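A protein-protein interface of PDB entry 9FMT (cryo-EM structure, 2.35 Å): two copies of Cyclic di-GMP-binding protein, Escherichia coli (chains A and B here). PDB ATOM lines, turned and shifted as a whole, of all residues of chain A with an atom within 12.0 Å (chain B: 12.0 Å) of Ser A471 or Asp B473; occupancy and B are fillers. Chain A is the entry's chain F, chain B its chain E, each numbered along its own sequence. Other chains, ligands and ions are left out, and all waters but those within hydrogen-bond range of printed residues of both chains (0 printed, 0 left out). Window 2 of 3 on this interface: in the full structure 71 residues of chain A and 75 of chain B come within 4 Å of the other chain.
The backbone carbonyl oxygen of Gly A470 is in hydrogen-bond range of the backbone NH of Cys B475 (3.0 Å).
N of Met A467 is in hydrogen-bond range of O of Thr B477 (2.6 Å).
The backbone carbonyl oxygen of Gly A470 lies close to the backbone carbonyl oxygen of Asp B473, at 3.0 Å.
The backbone carbonyl oxygen of Pro A468 lies within hydrogen-bond range of the backbone NH of Cys B157, at 3.2 Å.
SD of Met A467 sits close to O of Glu B158 (3.3 Å).
N of Ile A476 is in hydrogen-bond range of O of Gly A469 (2.7 Å).
The side-chain hydroxyl (OG) of Ser B471 sits close to the backbone NH (N) of Asp B473 (3.4 Å).
The backbone carbonyl oxygen (O) of Val A156 lies close to the side-chain amide oxygen (OE1) of Gln A154, 3.3 Å away.
NE2 of Gln B154 lies within hydrogen-bond range of O of Cys B157.
OD1 of Asp A473 lies within hydrogen-bond range of OG of Ser A471.
OG of Ser B471 sits at hydrogen-bond distance from N of Asn B474 (3.1 Å).
Pro B468 touches Ala A424.
CD2 of Leu A428 touches O of Cys B475, at 3.2 Å.
Ile B476 touches Met A467 (CD1 to O, 3.7 Å).
Pro A468 touches Asp B155 (CB to O, 3.7 Å).
O of Pro A468 touches CA of Val B156, 3.9 Å away.
CG1 of Val B156 touches O of Gly A469, at 3.3 Å.
SG of Cys B475 touches CA of Gly A469 (3.6 Å).
O of Gly A470 touches CA of Asn B474, 3.7 Å away.
Ser A471 touches Asp B473.
Phe A478 touches Ile B476 (CZ to CD1, 3.5 Å).
Printed residues of chain B within 4 Å of Ser A471: Val B156 and Asp B473.
Of chain A, only Gly A470 and Ser A471 come within 4 Å of Asp B473.
Gly A470 touches just these residues of chain B: Asp B473 (3.0 Å), Asn B474 (3.7 Å) and Cys B475 (3.0 Å).
No residue of chain B comes within 4 Å of Val A472.
No residue of chain B comes within 4 Å of Asp A473.
No residue of chain B comes within 4 Å of Asn A474.
No residue of chain B comes within 4 Å of Ile A476.
Val B156 touches just these residues of chain A: Pro A468, Gly A469, Ser A471 and Cys A475.
No residue of chain A comes within 4 Å of Ser B471.
No residue of chain A comes within 4 Å of Val B472.
Asn B474 touches two residues of chain A.
Of the printed residues of chain A, Asp B155 touches Gln A154 and Pro A468.
Printed residues of chain B within 4 Å of Phe A478: Ile B476.
Of the printed residues of chain A, Thr B477 touches Met A467.
The nearest residue of chain B that does not touch Ser A471 is Cys B475 (4.9 Å).
The nearest residue of chain A that does not touch Asp B473 is Asn A474 (6.0 Å).
The nearest printed residue of chain B that does not touch Pro A468 is Cys B475 (4.7 Å).
Of the 23 printed residues of chain A, 10 touch a printed residue of chain B.
Hydrophobic or aromatic side chains of chain A that line the printed part of chain B: Ala A424, Leu A428, Met A467, Pro A468 and Phe A478.
Among the printed residues, 19 pairs touch across the chains.
Gly A469 touches Cys B475, but with the chains exchanged Cys A475 does not touch Gly B469 (13.0 Å).
Gly A470 touches Asp B473, but with the chains exchanged Asp A473 does not touch Gly B470 (14.4 Å).
Gly A470 touches Asn B474, but with the chains exchanged Asn A474 does not touch Gly B470 (12.5 Å).
Ser A471 touches Val B156, but with the chains exchanged Val A156 does not touch Ser B471 (18.8 Å).
14 positions are printed for both chains.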
ATOM      1  N   GLN A 154      14.110  19.489  18.267  1.00  0.00           N
ATOM      2  CA  GLN A 154      13.856  19.563  19.697  1.00  0.00           C
ATOM      3  C   GLN A 154      14.819  20.563  20.316  1.00  0.00           C
ATOM      4  O   GLN A 154      15.836  20.926  19.721  1.00  0.00           O
ATOM      5  CB  GLN A 154      14.001  18.193  20.369  1.00  0.00           C
ATOM      6  CG  GLN A 154      12.689  17.553  20.764  1.00  0.00           C
ATOM      7  CD  GLN A 154      12.880  16.198  21.407  1.00  0.00           C
ATOM      8  OE1 GLN A 154      14.006  15.748  21.609  1.00  0.00           O
ATOM      9  NE2 GLN A 154      11.776  15.535  21.729  1.00  0.00           N
ATOM     10  N   VAL A 156      15.757  20.131  23.849  1.00  0.00           N
ATOM     11  CA  VAL A 156      16.476  19.416  24.895  1.00  0.00           C
ATOM     12  C   VAL A 156      16.784  18.013  24.393  1.00  0.00           C
ATOM     13  O   VAL A 156      15.897  17.331  23.866  1.00  0.00           O
ATOM     14  CB  VAL A 156      15.668  19.365  26.206  1.00  0.00           C
ATOM     15  CG1 VAL A 156      16.437  18.608  27.278  1.00  0.00           C
ATOM     16  CG2 VAL A 156      15.330  20.772  26.676  1.00  0.00           C
ATOM     17  N   CYS A 157      18.040  17.591  24.555  1.00  0.00           N
ATOM     18  CA  CYS A 157      18.498  16.261  24.148  1.00  0.00           C
ATOM     19  C   CYS A 157      18.285  16.035  22.652  1.00  0.00           C
ATOM     20  O   CYS A 157      17.772  15.002  22.220  1.00  0.00           O
ATOM     21  CB  CYS A 157      17.817  15.166  24.974  1.00  0.00           C
ATOM     22  SG  CYS A 157      18.076  15.326  26.752  1.00  0.00           S
ATOM     23  N   GLU A 158      18.690  17.020  21.857  1.00  0.00           N
ATOM     24  CA  GLU A 158      18.602  16.913  20.411  1.00  0.00           C
ATOM     25  C   GLU A 158      19.725  16.039  19.870  1.00  0.00           C
ATOM     26  O   GLU A 158      20.874  16.134  20.311  1.00  0.00           O
ATOM     27  CB  GLU A 158      18.668  18.298  19.768  1.00  0.00           C
ATOM     28  CG  GLU A 158      18.524  18.284  18.259  1.00  0.00           C
ATOM     29  CD  GLU A 158      17.686  19.433  17.747  1.00  0.00           C
ATOM     30  OE1 GLU A 158      18.081  20.599  17.960  1.00  0.00           O
ATOM     31  OE2 GLU A 158      16.630  19.172  17.137  1.00  0.00           O
ATOM     32  N   ALA A 424      34.241   3.762  25.488  1.00  0.00           N
ATOM     33  CA  ALA A 424      32.864   4.245  25.490  1.00  0.00           C
ATOM     34  C   ALA A 424      32.499   4.910  26.810  1.00  0.00           C
ATOM     35  O   ALA A 424      31.813   5.939  26.822  1.00  0.00           O
ATOM     36  CB  ALA A 424      31.907   3.095  25.192  1.00  0.00           C
ATOM     37  N   ASN A 425      32.936   4.336  27.933  1.00  0.00           N
ATOM     38  CA  ASN A 425      32.577   4.895  29.233  1.00  0.00           C
ATOM     39  C   ASN A 425      33.169   6.283  29.434  1.00  0.00           C
ATOM     40  O   ASN A 425      32.517   7.153  30.021  1.00  0.00           O
ATOM     41  CB  ASN A 425      33.024   3.954  30.352  1.00  0.00           C
ATOM     42  CG  ASN A 425      34.335   3.264  30.046  1.00  0.00           C
ATOM     43  OD1 ASN A 425      34.474   2.597  29.022  1.00  0.00           O
ATOM     44  ND2 ASN A 425      35.307   3.420  30.935  1.00  0.00           N
ATOM     45  N   ARG A 426      34.396   6.513  28.961  1.00  0.00           N
ATOM     46  CA  ARG A 426      35.008   7.829  29.094  1.00  0.00           C
ATOM     47  C   ARG A 426      34.303   8.889  28.260  1.00  0.00           C
ATOM     48  O   ARG A 426      34.434  10.080  28.560  1.00  0.00           O
ATOM     49  CB  ARG A 426      36.484   7.776  28.699  1.00  0.00           C
ATOM     50  CG  ARG A 426      37.413   7.251  29.779  1.00  0.00           C
ATOM     51  CD  ARG A 426      38.723   8.028  29.780  1.00  0.00           C
ATOM     52  NE  ARG A 426      39.850   7.223  30.234  1.00  0.00           N
ATOM     53  CZ  ARG A 426      41.047   7.221  29.661  1.00  0.00           C
ATOM     54  NH1 ARG A 426      41.310   7.978  28.608  1.00  0.00           N
ATOM     55  NH2 ARG A 426      42.003   6.444  30.159  1.00  0.00           N
ATOM     56  N   LEU A 427      33.564   8.487  27.225  1.00  0.00           N
ATOM     57  CA  LEU A 427      32.927   9.463  26.348  1.00  0.00           C
ATOM     58  C   LEU A 427      31.830  10.239  27.063  1.00  0.00           C
ATOM     59  O   LEU A 427      31.607  11.416  26.759  1.00  0.00           O
ATOM     60  CB  LEU A 427      32.361   8.765  25.112  1.00  0.00           C
ATOM     61  CG  LEU A 427      32.631   9.441  23.768  1.00  0.00           C
ATOM     62  CD1 LEU A 427      34.039  10.013  23.724  1.00  0.00           C
ATOM     63  CD2 LEU A 427      32.414   8.463  22.628  1.00  0.00           C
ATOM     64  N   LEU A 428      31.135   9.602  28.008  1.00  0.00           N
ATOM     65  CA  LEU A 428      30.064  10.279  28.728  1.00  0.00           C
ATOM     66  C   LEU A 428      30.577  11.392  29.630  1.00  0.00           C
ATOM     67  O   LEU A 428      29.799  12.273  30.008  1.00  0.00           O
ATOM     68  CB  LEU A 428      29.267   9.267  29.549  1.00  0.00           C
ATOM     69  CG  LEU A 428      28.302   8.400  28.743  1.00  0.00           C
ATOM     70  CD1 LEU A 428      28.198   7.013  29.346  1.00  0.00           C
ATOM     71  CD2 LEU A 428      26.939   9.060  28.664  1.00  0.00           C
ATOM     72  N   LEU A 429      31.864  11.376  29.983  1.00  0.00           N
ATOM     73  CA  LEU A 429      32.421  12.440  30.809  1.00  0.00           C
ATOM     74  C   LEU A 429      32.568  13.746  30.042  1.00  0.00           C
ATOM     75  O   LEU A 429      32.716  14.801  30.670  1.00  0.00           O
ATOM     76  CB  LEU A 429      33.775  12.011  31.374  1.00  0.00           C
ATOM     77  CG  LEU A 429      33.831  10.627  32.023  1.00  0.00           C
ATOM     78  CD1 LEU A 429      35.212  10.358  32.599  1.00  0.00           C
ATOM     79  CD2 LEU A 429      32.762  10.490  33.096  1.00  0.00           C
ATOM     80  N   ARG A 430      32.527  13.697  28.710  1.00  0.00           N
ATOM     81  CA  ARG A 430      32.631  14.884  27.860  1.00  0.00           C
ATOM     82  C   ARG A 430      33.897  15.682  28.162  1.00  0.00           C
ATOM     83  O   ARG A 430      33.880  16.913  28.213  1.00  0.00           O
ATOM     84  CB  ARG A 430      31.388  15.769  27.985  1.00  0.00           C
ATOM     85  CG  ARG A 430      30.431  15.650  26.809  1.00  0.00           C
ATOM     86  CD  ARG A 430      29.173  16.471  27.030  1.00  0.00           C
ATOM     87  NE  ARG A 430      28.744  16.458  28.423  1.00  0.00           N
ATOM     88  CZ  ARG A 430      27.843  17.284  28.936  1.00  0.00           C
ATOM     89  NH1 ARG A 430      27.257  18.212  28.199  1.00  0.00           N
ATOM     90  NH2 ARG A 430      27.522  17.175  30.222  1.00  0.00           N
ATOM     91  N   MET A 467      25.277   8.595  20.137  1.00  0.00           N
ATOM     92  CA  MET A 467      23.937   9.134  20.280  1.00  0.00           C
ATOM     93  C   MET A 467      23.756   9.693  21.684  1.00  0.00           C
ATOM     94  O   MET A 467      24.554   9.400  22.581  1.00  0.00           O
ATOM     95  CB  MET A 467      22.887   8.049  20.010  1.00  0.00           C
ATOM     96  CG  MET A 467      22.656   7.763  18.538  1.00  0.00           C
ATOM     97  SD  MET A 467      21.627   6.312  18.271  1.00  0.00           S
ATOM     98  CE  MET A 467      20.008   7.068  18.146  1.00  0.00           C
ATOM     99  N   PRO A 468      22.737  10.525  21.910  1.00  0.00           N
ATOM    100  CA  PRO A 468      22.510  11.056  23.259  1.00  0.00           C
ATOM    101  C   PRO A 468      22.389   9.942  24.289  1.00  0.00           C
ATOM    102  O   PRO A 468      21.709   8.938  24.073  1.00  0.00           O
ATOM    103  CB  PRO A 468      21.199  11.830  23.111  1.00  0.00           C
ATOM    104  CG  PRO A 468      21.206  12.281  21.704  1.00  0.00           C
ATOM    105  CD  PRO A 468      21.897  11.205  20.909  1.00  0.00           C
ATOM    106  N   GLY A 469      23.062  10.129  25.422  1.00  0.00           N
ATOM    107  CA  GLY A 469      23.133   9.098  26.435  1.00  0.00           C
ATOM    108  C   GLY A 469      23.034   9.616  27.853  1.00  0.00           C
ATOM    109  O   GLY A 469      22.545  10.724  28.087  1.00  0.00           O
ATOM    110  N   GLY A 470      23.497   8.816  28.810  1.00  0.00           N
ATOM    111  CA  GLY A 470      23.383   9.161  30.211  1.00  0.00           C
ATOM    112  C   GLY A 470      22.254   8.420  30.896  1.00  0.00           C
ATOM    113  O   GLY A 470      22.363   7.220  31.164  1.00  0.00           O
ATOM    114  N   SER A 471      21.164   9.124  31.181  1.00  0.00           N
ATOM    115  CA  SER A 471      19.992   8.526  31.805  1.00  0.00           C
ATOM    116  C   SER A 471      18.782   9.383  31.456  1.00  0.00           C
ATOM    117  O   SER A 471      18.897  10.401  30.767  1.00  0.00           O
ATOM    118  CB  SER A 471      20.174   8.395  33.320  1.00  0.00           C
ATOM    119  OG  SER A 471      20.765   9.560  33.866  1.00  0.00           O
ATOM    120  N   VAL A 472      17.611   8.955  31.928  1.00  0.00           N
ATOM    121  CA  VAL A 472      16.388   9.706  31.664  1.00  0.00           C
ATOM    122  C   VAL A 472      16.446  11.072  32.335  1.00  0.00           C
ATOM    123  O   VAL A 472      16.136  12.098  31.719  1.00  0.00           O
ATOM    124  CB  VAL A 472      15.158   8.902  32.120  1.00  0.00           C
ATOM    125  CG1 VAL A 472      13.905   9.418  31.432  1.00  0.00           C
ATOM    126  CG2 VAL A 472      15.358   7.422  31.840  1.00  0.00           C
ATOM    127  N   ASP A 473      16.844  11.107  33.609  1.00  0.00           N
ATOM    128  CA  ASP A 473      16.951  12.384  34.310  1.00  0.00           C
ATOM    129  C   ASP A 473      18.185  13.160  33.866  1.00  0.00           C
ATOM    130  O   ASP A 473      18.116  14.376  33.654  1.00  0.00           O
ATOM    131  CB  ASP A 473      16.976  12.155  35.821  1.00  0.00           C
ATOM    132  CG  ASP A 473      17.947  11.065  36.232  1.00  0.00           C
ATOM    133  OD1 ASP A 473      18.442  10.341  35.343  1.00  0.00           O
ATOM    134  OD2 ASP A 473      18.217  10.934  37.444  1.00  0.00           O
ATOM    135  N   ASN A 474      19.318  12.481  33.719  1.00  0.00           N
ATOM    136  CA  ASN A 474      20.574  13.103  33.317  1.00  0.00           C
ATOM    137  C   ASN A 474      20.887  12.668  31.892  1.00  0.00           C
ATOM    138  O   ASN A 474      21.326  11.536  31.665  1.00  0.00           O
ATOM    139  CB  ASN A 474      21.705  12.721  34.271  1.00  0.00           C
ATOM    140  CG  ASN A 474      23.038  13.310  33.860  1.00  0.00           C
ATOM    141  OD1 ASN A 474      23.099  14.396  33.284  1.00  0.00           O
ATOM    142  ND2 ASN A 474      24.117  12.594  34.154  1.00  0.00           N
ATOM    143  N   CYS A 475      20.672  13.568  30.939  1.00  0.00           N
ATOM    144  CA  CYS A 475      20.840  13.281  29.521  1.00  0.00           C
ATOM    145  C   CYS A 475      22.048  14.048  29.002  1.00  0.00           C
ATOM    146  O   CYS A 475      22.118  15.274  29.139  1.00  0.00           O
ATOM    147  CB  CYS A 475      19.575  13.648  28.745  1.00  0.00           C
ATOM    148  SG  CYS A 475      19.824  14.354  27.106  1.00  0.00           S
ATOM    149  N   ILE A 476      22.997  13.324  28.413  1.00  0.00           N
ATOM    150  CA  ILE A 476      24.254  13.887  27.938  1.00  0.00           C
ATOM    151  C   ILE A 476      24.239  13.882  26.417  1.00  0.00           C
ATOM    152  O   ILE A 476      24.004  12.839  25.795  1.00  0.00           O
ATOM    153  CB  ILE A 476      25.460  13.099  28.478  1.00  0.00           C
ATOM    154  CG1 ILE A 476      25.343  12.920  29.992  1.00  0.00           C
ATOM    155  CG2 ILE A 476      26.757  13.798  28.116  1.00  0.00           C
ATOM    156  CD1 ILE A 476      26.527  12.225  30.621  1.00  0.00           C
ATOM    157  N   THR A 477      24.489  15.043  25.822  1.00  0.00           N
ATOM    158  CA  THR A 477      24.497  15.204  24.376  1.00  0.00           C
ATOM    159  C   THR A 477      25.907  15.522  23.904  1.00  0.00           C
ATOM    160  O   THR A 477      26.634  16.281  24.552  1.00  0.00           O
ATOM    161  CB  THR A 477      23.542  16.313  23.933  1.00  0.00           C
ATOM    162  OG1 THR A 477      23.688  17.446  24.798  1.00  0.00           O
ATOM    163  CG2 THR A 477      22.108  15.825  23.985  1.00  0.00           C
ATOM    164  N   PHE A 478      26.286  14.938  22.773  1.00  0.00           N
ATOM    165  CA  PHE A 478      27.606  15.130  22.190  1.00  0.00           C
ATOM    166  C   PHE A 478      27.496  16.066  20.997  1.00  0.00           C
ATOM    167  O   PHE A 478      26.705  15.821  20.080  1.00  0.00           O
ATOM    168  CB  PHE A 478      28.218  13.793  21.763  1.00  0.00           C
ATOM    169  CG  PHE A 478      28.144  12.729  22.819  1.00  0.00           C
ATOM    170  CD1 PHE A 478      27.039  11.901  22.912  1.00  0.00           C
ATOM    171  CD2 PHE A 478      29.180  12.556  23.721  1.00  0.00           C
ATOM    172  CE1 PHE A 478      26.971  10.925  23.884  1.00  0.00           C
ATOM    173  CE2 PHE A 478      29.115  11.581  24.693  1.00  0.00           C
ATOM    174  CZ  PHE A 478      28.010  10.765  24.774  1.00  0.00           C
ATOM    175  N   GLN B 154      12.748   6.639  21.626  1.00  0.00           N
ATOM    176  CA  GLN B 154      13.324   7.173  22.850  1.00  0.00           C
ATOM    177  C   GLN B 154      14.184   8.379  22.511  1.00  0.00           C
ATOM    178  O   GLN B 154      14.624   8.555  21.373  1.00  0.00           O
ATOM    179  CB  GLN B 154      14.155   6.116  23.582  1.00  0.00           C
ATOM    180  CG  GLN B 154      13.559   5.645  24.890  1.00  0.00           C
ATOM    181  CD  GLN B 154      14.377   4.546  25.531  1.00  0.00           C
ATOM    182  OE1 GLN B 154      13.849   3.705  26.254  1.00  0.00           O
ATOM    183  NE2 GLN B 154      15.675   4.539  25.258  1.00  0.00           N
ATOM    184  N   ASP B 155      14.417   9.210  23.525  1.00  0.00           N
ATOM    185  CA  ASP B 155      15.321  10.346  23.405  1.00  0.00           C
ATOM    186  C   ASP B 155      16.718  10.047  23.921  1.00  0.00           C
ATOM    187  O   ASP B 155      17.689  10.616  23.411  1.00  0.00           O
ATOM    188  CB  ASP B 155      14.757  11.555  24.158  1.00  0.00           C
ATOM    189  CG  ASP B 155      13.554  12.163  23.469  1.00  0.00           C
ATOM    190  OD1 ASP B 155      13.303  11.821  22.294  1.00  0.00           O
ATOM    191  OD2 ASP B 155      12.858  12.985  24.102  1.00  0.00           O
ATOM    192  N   VAL B 156      16.841   9.172  24.914  1.00  0.00           N
ATOM    193  CA  VAL B 156      18.119   8.811  25.515  1.00  0.00           C
ATOM    194  C   VAL B 156      18.286   7.304  25.397  1.00  0.00           C
ATOM    195  O   VAL B 156      17.346   6.551  25.675  1.00  0.00           O
ATOM    196  CB  VAL B 156      18.202   9.257  26.986  1.00  0.00           C
ATOM    197  CG1 VAL B 156      19.639   9.273  27.454  1.00  0.00           C
ATOM    198  CG2 VAL B 156      17.568  10.626  27.170  1.00  0.00           C
ATOM    199  N   CYS B 157      19.480   6.869  24.987  1.00  0.00           N
ATOM    200  CA  CYS B 157      19.803   5.449  24.828  1.00  0.00           C
ATOM    201  C   CYS B 157      18.857   4.771  23.837  1.00  0.00           C
ATOM    202  O   CYS B 157      18.232   3.751  24.138  1.00  0.00           O
ATOM    203  CB  CYS B 157      19.791   4.713  26.172  1.00  0.00           C
ATOM    204  SG  CYS B 157      20.125   5.717  27.633  1.00  0.00           S
ATOM    205  N   GLU B 158      18.753   5.345  22.644  1.00  0.00           N
ATOM    206  CA  GLU B 158      17.897   4.799  21.596  1.00  0.00           C
ATOM    207  C   GLU B 158      18.718   3.848  20.734  1.00  0.00           C
ATOM    208  O   GLU B 158      19.608   4.280  19.996  1.00  0.00           O
ATOM    209  CB  GLU B 158      17.290   5.915  20.752  1.00  0.00           C
ATOM    210  CG  GLU B 158      16.318   5.417  19.698  1.00  0.00           C
ATOM    211  CD  GLU B 158      16.099   6.420  18.588  1.00  0.00           C
ATOM    212  OE1 GLU B 158      15.324   7.377  18.793  1.00  0.00           O
ATOM    213  OE2 GLU B 158      16.702   6.253  17.507  1.00  0.00           O
ATOM    214  N   PRO B 468      29.336  -0.899  22.039  1.00  0.00           N
ATOM    215  CA  PRO B 468      29.514  -0.614  23.466  1.00  0.00           C
ATOM    216  C   PRO B 468      28.320   0.145  24.025  1.00  0.00           C
ATOM    217  O   PRO B 468      27.720   0.982  23.348  1.00  0.00           O
ATOM    218  CB  PRO B 468      30.793   0.231  23.503  1.00  0.00           C
ATOM    219  CG  PRO B 468      31.461  -0.006  22.188  1.00  0.00           C
ATOM    220  CD  PRO B 468      30.363  -0.251  21.210  1.00  0.00           C
ATOM    221  N   GLY B 469      27.977  -0.155  25.274  1.00  0.00           N
ATOM    222  CA  GLY B 469      26.783   0.407  25.872  1.00  0.00           C
ATOM    223  C   GLY B 469      26.984   1.019  27.241  1.00  0.00           C
ATOM    224  O   GLY B 469      26.021   1.465  27.870  1.00  0.00           O
ATOM    225  N   GLY B 470      28.227   1.058  27.709  1.00  0.00           N
ATOM    226  CA  GLY B 470      28.491   1.611  29.027  1.00  0.00           C
ATOM    227  C   GLY B 470      27.837   0.780  30.111  1.00  0.00           C
ATOM    228  O   GLY B 470      28.038  -0.435  30.203  1.00  0.00           O
ATOM    229  N   SER B 471      27.041   1.438  30.949  1.00  0.00           N
ATOM    230  CA  SER B 471      26.317   0.788  32.029  1.00  0.00           C
ATOM    231  C   SER B 471      24.869   1.254  32.013  1.00  0.00           C
ATOM    232  O   SER B 471      24.484   2.129  31.233  1.00  0.00           O
ATOM    233  CB  SER B 471      26.959   1.080  33.392  1.00  0.00           C
ATOM    234  OG  SER B 471      26.655   2.393  33.826  1.00  0.00           O
ATOM    235  N   VAL B 472      24.057   0.646  32.880  1.00  0.00           N
ATOM    236  CA  VAL B 472      22.656   1.043  32.985  1.00  0.00           C
ATOM    237  C   VAL B 472      22.544   2.479  33.480  1.00  0.00           C
ATOM    238  O   VAL B 472      21.760   3.276  32.950  1.00  0.00           O
ATOM    239  CB  VAL B 472      21.891   0.063  33.894  1.00  0.00           C
ATOM    240  CG1 VAL B 472      20.624   0.709  34.437  1.00  0.00           C
ATOM    241  CG2 VAL B 472      21.563  -1.211  33.136  1.00  0.00           C
ATOM    242  N   ASP B 473      23.329   2.835  34.498  1.00  0.00           N
ATOM    243  CA  ASP B 473      23.296   4.200  35.014  1.00  0.00           C
ATOM    244  C   ASP B 473      23.828   5.196  33.990  1.00  0.00           C
ATOM    245  O   ASP B 473      23.273   6.290  33.833  1.00  0.00           O
ATOM    246  CB  ASP B 473      24.095   4.291  36.313  1.00  0.00           C
ATOM    247  CG  ASP B 473      23.495   3.455  37.427  1.00  0.00           C
ATOM    248  OD1 ASP B 473      22.335   3.015  37.284  1.00  0.00           O
ATOM    249  OD2 ASP B 473      24.183   3.240  38.447  1.00  0.00           O
ATOM    250  N   ASN B 474      24.898   4.838  33.285  1.00  0.00           N
ATOM    251  CA  ASN B 474      25.524   5.698  32.283  1.00  0.00           C
ATOM    252  C   ASN B 474      25.480   4.968  30.944  1.00  0.00           C
ATOM    253  O   ASN B 474      26.418   4.257  30.576  1.00  0.00           O
ATOM    254  CB  ASN B 474      26.951   6.056  32.680  1.00  0.00           C
ATOM    255  CG  ASN B 474      27.019   7.299  33.539  1.00  0.00           C
ATOM    256  OD1 ASN B 474      26.118   8.135  33.513  1.00  0.00           O
ATOM    257  ND2 ASN B 474      28.093   7.426  34.310  1.00  0.00           N
ATOM    258  N   CYS B 475      24.383   5.149  30.216  1.00  0.00           N
ATOM    259  CA  CYS B 475      24.189   4.493  28.934  1.00  0.00           C
ATOM    260  C   CYS B 475      24.941   5.225  27.828  1.00  0.00           C
ATOM    261  O   CYS B 475      25.267   6.408  27.935  1.00  0.00           O
ATOM    262  CB  CYS B 475      22.704   4.433  28.583  1.00  0.00           C
ATOM    263  SG  CYS B 475      22.145   5.878  27.657  1.00  0.00           S
ATOM    264  N   ILE B 476      25.214   4.496  26.751  1.00  0.00           N
ATOM    265  CA  ILE B 476      25.754   5.083  25.530  1.00  0.00           C
ATOM    266  C   ILE B 476      25.318   4.216  24.357  1.00  0.00           C
ATOM    267  O   ILE B 476      25.330   2.985  24.437  1.00  0.00           O
ATOM    268  CB  ILE B 476      27.291   5.241  25.601  1.00  0.00           C
ATOM    269  CG1 ILE B 476      27.808   6.032  24.400  1.00  0.00           C
ATOM    270  CG2 ILE B 476      27.987   3.894  25.698  1.00  0.00           C
ATOM    271  CD1 ILE B 476      27.152   7.374  24.230  1.00  0.00           C
ATOM    272  N   THR B 477      24.900   4.868  23.276  1.00  0.00           N
ATOM    273  CA  THR B 477      24.446   4.184  22.075  1.00  0.00           C
ATOM    274  C   THR B 477      25.069   4.851  20.859  1.00  0.00           C
ATOM    275  O   THR B 477      25.315   6.059  20.853  1.00  0.00           O
ATOM    276  CB  THR B 477      22.916   4.198  21.963  1.00  0.00           C
ATOM    277  OG1 THR B 477      22.342   3.887  23.238  1.00  0.00           O
ATOM    278  CG2 THR B 477      22.448   3.166  20.954  1.00  0.00           C
